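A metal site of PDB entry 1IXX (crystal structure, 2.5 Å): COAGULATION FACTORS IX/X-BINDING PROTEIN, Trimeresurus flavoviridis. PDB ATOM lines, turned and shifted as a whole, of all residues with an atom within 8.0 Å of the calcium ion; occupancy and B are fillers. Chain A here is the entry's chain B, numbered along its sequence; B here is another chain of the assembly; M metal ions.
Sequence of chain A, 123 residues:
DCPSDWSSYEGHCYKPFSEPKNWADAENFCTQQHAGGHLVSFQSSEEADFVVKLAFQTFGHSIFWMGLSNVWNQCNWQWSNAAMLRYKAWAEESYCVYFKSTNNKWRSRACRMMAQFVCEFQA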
ATOM      1  N   TYR A   9     -11.552   2.731  -9.199  1.00  0.00           N
ATOM      2  CA  TYR A   9     -11.067   4.091  -9.137  1.00  0.00           C
ATOM      3  C   TYR A   9     -10.293   4.202  -7.827  1.00  0.00           C
ATOM      4  O   TYR A   9     -10.820   3.831  -6.771  1.00  0.00           O
ATOM      5  CB  TYR A   9     -12.208   5.114  -9.190  1.00  0.00           C
ATOM      6  CG  TYR A   9     -11.772   6.543  -8.952  1.00  0.00           C
ATOM      7  CD1 TYR A   9     -11.239   7.327  -9.983  1.00  0.00           C
ATOM      8  CD2 TYR A   9     -11.819   7.098  -7.676  1.00  0.00           C
ATOM      9  CE1 TYR A   9     -10.771   8.609  -9.746  1.00  0.00           C
ATOM     10  CE2 TYR A   9     -11.352   8.379  -7.417  1.00  0.00           C
ATOM     11  CZ  TYR A   9     -10.825   9.124  -8.450  1.00  0.00           C
ATOM     12  OH  TYR A   9     -10.333  10.390  -8.178  1.00  0.00           O
ATOM     13  N   HIS A  12     -10.507   1.498  -5.240  1.00  0.00           N
ATOM     14  CA  HIS A  12     -11.860   1.218  -4.777  1.00  0.00           C
ATOM     15  C   HIS A  12     -12.661   0.594  -5.894  1.00  0.00           C
ATOM     16  O   HIS A  12     -12.345   0.782  -7.070  1.00  0.00           O
ATOM     17  CB  HIS A  12     -12.547   2.507  -4.321  1.00  0.00           C
ATOM     18  CG  HIS A  12     -12.112   2.973  -2.966  1.00  0.00           C
ATOM     19  ND1 HIS A  12     -10.864   3.515  -2.742  1.00  0.00           N
ATOM     20  CD2 HIS A  12     -12.756   2.978  -1.779  1.00  0.00           C
ATOM     21  CE1 HIS A  12     -10.753   3.813  -1.465  1.00  0.00           C
ATOM     22  NE2 HIS A  12     -11.879   3.500  -0.857  1.00  0.00           N
ATOM     23  N   TYR A  14     -16.535   0.171  -7.441  1.00  0.00           N
ATOM     24  CA  TYR A  14     -17.825   0.839  -7.427  1.00  0.00           C
ATOM     25  C   TYR A  14     -18.793   0.109  -8.358  1.00  0.00           C
ATOM     26  O   TYR A  14     -18.365  -0.503  -9.336  1.00  0.00           O
ATOM     27  CB  TYR A  14     -17.690   2.294  -7.920  1.00  0.00           C
ATOM     28  CG  TYR A  14     -16.666   3.138  -7.201  1.00  0.00           C
ATOM     29  CD1 TYR A  14     -15.309   3.066  -7.537  1.00  0.00           C
ATOM     30  CD2 TYR A  14     -17.047   4.025  -6.194  1.00  0.00           C
ATOM     31  CE1 TYR A  14     -14.362   3.866  -6.904  1.00  0.00           C
ATOM     32  CE2 TYR A  14     -16.108   4.835  -5.543  1.00  0.00           C
ATOM     33  CZ  TYR A  14     -14.763   4.746  -5.907  1.00  0.00           C
ATOM     34  OH  TYR A  14     -13.832   5.528  -5.271  1.00  0.00           O
ATOM     35  N   LEU A  39     -22.692   2.376   0.792  1.00  0.00           N
ATOM     36  CA  LEU A  39     -23.213   3.255  -0.241  1.00  0.00           C
ATOM     37  C   LEU A  39     -22.020   4.151  -0.580  1.00  0.00           C
ATOM     38  O   LEU A  39     -21.209   4.452   0.301  1.00  0.00           O
ATOM     39  CB  LEU A  39     -24.368   4.073   0.341  1.00  0.00           C
ATOM     40  CG  LEU A  39     -25.690   4.260  -0.409  1.00  0.00           C
ATOM     41  CD1 LEU A  39     -25.768   3.355  -1.617  1.00  0.00           C
ATOM     42  CD2 LEU A  39     -26.844   4.033   0.556  1.00  0.00           C
ATOM     43  N   VAL A  40     -21.911   4.567  -1.828  1.00  0.00           N
ATOM     44  CA  VAL A  40     -20.782   5.387  -2.267  1.00  0.00           C
ATOM     45  C   VAL A  40     -20.539   6.641  -1.413  1.00  0.00           C
ATOM     46  O   VAL A  40     -21.466   7.211  -0.849  1.00  0.00           O
ATOM     47  CB  VAL A  40     -20.949   5.789  -3.754  1.00  0.00           C
ATOM     48  CG1 VAL A  40     -22.053   6.801  -3.900  1.00  0.00           C
ATOM     49  CG2 VAL A  40     -19.636   6.314  -4.314  1.00  0.00           C
ATOM     50  N   SER A  41     -19.279   7.059  -1.361  1.00  0.00           N
ATOM     51  CA  SER A  41     -18.861   8.229  -0.603  1.00  0.00           C
ATOM     52  C   SER A  41     -17.931   9.063  -1.456  1.00  0.00           C
ATOM     53  O   SER A  41     -16.979   8.531  -2.053  1.00  0.00           O
ATOM     54  CB  SER A  41     -18.133   7.812   0.675  1.00  0.00           C
ATOM     55  OG  SER A  41     -16.878   7.216   0.367  1.00  0.00           O
ATOM     56  N   PHE A  42     -18.168  10.368  -1.485  1.00  0.00           N
ATOM     57  CA  PHE A  42     -17.346  11.276  -2.263  1.00  0.00           C
ATOM     58  C   PHE A  42     -16.309  11.946  -1.373  1.00  0.00           C
ATOM     59  O   PHE A  42     -16.618  12.442  -0.293  1.00  0.00           O
ATOM     60  CB  PHE A  42     -18.200  12.340  -2.957  1.00  0.00           C
ATOM     61  CG  PHE A  42     -19.179  11.788  -3.956  1.00  0.00           C
ATOM     62  CD1 PHE A  42     -19.131  10.452  -4.333  1.00  0.00           C
ATOM     63  CD2 PHE A  42     -20.128  12.617  -4.535  1.00  0.00           C
ATOM     64  CE1 PHE A  42     -20.029   9.965  -5.268  1.00  0.00           C
ATOM     65  CE2 PHE A  42     -21.028  12.120  -5.470  1.00  0.00           C
ATOM     66  CZ  PHE A  42     -20.974  10.793  -5.834  1.00  0.00           C
ATOM     67  N   GLN A  43     -15.058  11.928  -1.836  1.00  0.00           N
ATOM     68  CA  GLN A  43     -13.964  12.506  -1.083  1.00  0.00           C
ATOM     69  C   GLN A  43     -13.324  13.635  -1.874  1.00  0.00           C
ATOM     70  O   GLN A  43     -12.561  14.428  -1.328  1.00  0.00           O
ATOM     71  CB  GLN A  43     -12.925  11.432  -0.731  1.00  0.00           C
ATOM     72  CG  GLN A  43     -13.023  10.862   0.698  1.00  0.00           C
ATOM     73  CD  GLN A  43     -14.129   9.828   0.894  1.00  0.00           C
ATOM     74  OE1 GLN A  43     -14.404   8.997   0.010  1.00  0.00           O
ATOM     75  NE2 GLN A  43     -14.738   9.849   2.065  1.00  0.00           N
ATOM     76  N   SER A  44     -13.650  13.696  -3.164  1.00  0.00           N
ATOM     77  CA  SER A  44     -13.117  14.727  -4.066  1.00  0.00           C
ATOM     78  C   SER A  44     -14.045  14.867  -5.261  1.00  0.00           C
ATOM     79  O   SER A  44     -14.917  14.011  -5.478  1.00  0.00           O
ATOM     80  CB  SER A  44     -11.714  14.321  -4.560  1.00  0.00           C
ATOM     81  OG  SER A  44     -11.750  13.176  -5.398  1.00  0.00           O
ATOM     82  N   GLU A  47     -13.504  11.844  -7.891  1.00  0.00           N
ATOM     83  CA  GLU A  47     -14.215  10.641  -7.568  1.00  0.00           C
ATOM     84  C   GLU A  47     -15.676  10.826  -7.893  1.00  0.00           C
ATOM     85  O   GLU A  47     -16.323   9.911  -8.396  1.00  0.00           O
ATOM     86  CB  GLU A  47     -14.038  10.329  -6.090  1.00  0.00           C
ATOM     87  CG  GLU A  47     -14.716   9.063  -5.657  1.00  0.00           C
ATOM     88  CD  GLU A  47     -14.490   8.746  -4.208  1.00  0.00           C
ATOM     89  OE1 GLU A  47     -14.066   9.641  -3.450  1.00  0.00           O
ATOM     90  OE2 GLU A  47     -14.751   7.590  -3.826  1.00  0.00           O
ATOM     91  N   ALA A  48     -16.182  12.026  -7.610  1.00  0.00           N
ATOM     92  CA  ALA A  48     -17.584  12.341  -7.873  1.00  0.00           C
ATOM     93  C   ALA A  48     -17.877  12.286  -9.369  1.00  0.00           C
ATOM     94  O   ALA A  48     -18.858  11.682  -9.787  1.00  0.00           O
ATOM     95  CB  ALA A  48     -17.926  13.711  -7.302  1.00  0.00           C
ATOM     96  N   VAL A  51     -17.959   8.539 -10.484  1.00  0.00           N
ATOM     97  CA  VAL A  51     -19.184   7.839 -10.123  1.00  0.00           C
ATOM     98  C   VAL A  51     -20.404   8.326 -10.895  1.00  0.00           C
ATOM     99  O   VAL A  51     -21.224   7.505 -11.323  1.00  0.00           O
ATOM    100  CB  VAL A  51     -19.459   7.920  -8.592  1.00  0.00           C
ATOM    101  CG1 VAL A  51     -20.750   7.179  -8.231  1.00  0.00           C
ATOM    102  CG2 VAL A  51     -18.287   7.299  -7.842  1.00  0.00           C
ATOM    103  N   GLU A 120     -19.895   1.057  -2.924  1.00  0.00           N
ATOM    104  CA  GLU A 120     -18.463   1.251  -2.967  1.00  0.00           C
ATOM    105  C   GLU A 120     -17.813   0.392  -1.911  1.00  0.00           C
ATOM    106  O   GLU A 120     -18.398   0.142  -0.855  1.00  0.00           O
ATOM    107  CB  GLU A 120     -18.122   2.713  -2.690  1.00  0.00           C
ATOM    108  CG  GLU A 120     -16.636   2.969  -2.535  1.00  0.00           C
ATOM    109  CD  GLU A 120     -16.304   4.425  -2.308  1.00  0.00           C
ATOM    110  OE1 GLU A 120     -17.172   5.195  -1.866  1.00  0.00           O
ATOM    111  OE2 GLU A 120     -15.145   4.805  -2.571  1.00  0.00           O
ATOM    112  N   PHE A 121     -16.624  -0.102  -2.211  1.00  0.00           N
ATOM    113  CA  PHE A 121     -15.833  -0.865  -1.275  1.00  0.00           C
ATOM    114  C   PHE A 121     -14.363  -0.727  -1.705  1.00  0.00           C
ATOM    115  O   PHE A 121     -14.062  -0.278  -2.805  1.00  0.00           O
ATOM    116  CB  PHE A 121     -16.339  -2.316  -1.096  1.00  0.00           C
ATOM    117  CG  PHE A 121     -15.953  -3.249  -2.190  1.00  0.00           C
ATOM    118  CD1 PHE A 121     -14.644  -3.701  -2.314  1.00  0.00           C
ATOM    119  CD2 PHE A 121     -16.918  -3.718  -3.081  1.00  0.00           C
ATOM    120  CE1 PHE A 121     -14.286  -4.615  -3.310  1.00  0.00           C
ATOM    121  CE2 PHE A 121     -16.581  -4.629  -4.077  1.00  0.00           C
ATOM    122  CZ  PHE A 121     -15.253  -5.074  -4.191  1.00  0.00           C
ATOM    123  N   TRP B  83     -19.632   9.755   6.672  1.00  0.00           N
ATOM    124  CA  TRP B  83     -20.320   8.901   5.714  1.00  0.00           C
ATOM    125  C   TRP B  83     -20.540   7.541   6.374  1.00  0.00           C
ATOM    126  O   TRP B  83     -19.884   7.222   7.371  1.00  0.00           O
ATOM    127  CB  TRP B  83     -19.477   8.717   4.458  1.00  0.00           C
ATOM    128  CG  TRP B  83     -19.211   9.945   3.667  1.00  0.00           C
ATOM    129  CD1 TRP B  83     -18.141  10.774   3.787  1.00  0.00           C
ATOM    130  CD2 TRP B  83     -19.970  10.419   2.553  1.00  0.00           C
ATOM    131  NE1 TRP B  83     -18.179  11.736   2.807  1.00  0.00           N
ATOM    132  CE2 TRP B  83     -19.292  11.548   2.032  1.00  0.00           C
ATOM    133  CE3 TRP B  83     -21.159  10.011   1.926  1.00  0.00           C
ATOM    134  CZ2 TRP B  83     -19.756  12.259   0.922  1.00  0.00           C
ATOM    135  CZ3 TRP B  83     -21.620  10.711   0.828  1.00  0.00           C
ATOM    136  CH2 TRP B  83     -20.927  11.826   0.339  1.00  0.00           C
ATOM    137  N   ASP B  85     -19.408   4.816   5.710  1.00  0.00           N
ATOM    138  CA  ASP B  85     -18.212   3.989   5.730  1.00  0.00           C
ATOM    139  C   ASP B  85     -17.230   4.382   6.837  1.00  0.00           C
ATOM    140  O   ASP B  85     -16.131   3.840   6.921  1.00  0.00           O
ATOM    141  CB  ASP B  85     -17.527   4.017   4.371  1.00  0.00           C
ATOM    142  CG  ASP B  85     -17.077   5.418   3.959  1.00  0.00           C
ATOM    143  OD1 ASP B  85     -17.172   6.361   4.777  1.00  0.00           O
ATOM    144  OD2 ASP B  85     -16.610   5.560   2.809  1.00  0.00           O
ATOM    145  N   SER B  87     -15.720   7.401   7.174  1.00  0.00           N
ATOM    146  CA  SER B  87     -14.885   8.556   6.840  1.00  0.00           C
ATOM    147  C   SER B  87     -15.619   9.876   7.053  1.00  0.00           C
ATOM    148  O   SER B  87     -16.810   9.976   6.774  1.00  0.00           O
ATOM    149  CB  SER B  87     -14.361   8.462   5.397  1.00  0.00           C
ATOM    150  OG  SER B  87     -15.437   8.316   4.483  1.00  0.00           O
HETATM  151 CA    CA M   1     -15.209   7.212  -1.370  1.00  0.00          CA
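The side-chain hydroxyl of Tyr 9 is in hydrogen-bond range of the backbone NH of Glu 47 (3.5 Å). OG of Ser 44 sits at hydrogen-bond distance from N of Glu 47 (3.3 Å). The side-chain amide nitrogen (NE2) of Gln 43 sits at hydrogen-bond distance from the side-chain hydroxyl (OG) of Ser 87 of chain B (2.9 Å). OH of Tyr 14 sits close to OE2 of Glu 120. OE2 of Glu 47 sits close to OH of Tyr 14, 2.7 Å away. OG of Ser 41 sits close to OD2 of Asp 85 of chain B, at 3.0 Å.
Of the 17 residues printed, 4 come within 4 Å of the calcium ion. Along chain A the residues within 4 Å of the calcium ion span positions 41 to 120. The nearest printed residue that does not touch the calcium ion is Phe 42 (4.3 Å).
The calcium ion is bound by O of Ser 41 (2.3 Å). The side-chain amide oxygen (OE1) of Gln 43 is bound to the calcium ion (2.4 Å). OG of Ser 41 binds the calcium ion (2.4 Å). The calcium ion is bound by the side-chain carboxylate (OE2) of Glu 47, at 2.5 Å. The side-chain carboxylate (OE2) of Glu 120 binds the calcium ion (2.7 Å). The calcium ion is bound by the side-chain carboxylate (OE1) of Glu 120 (2.9 Å). The calcium ion has six donor atoms within binding distance.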
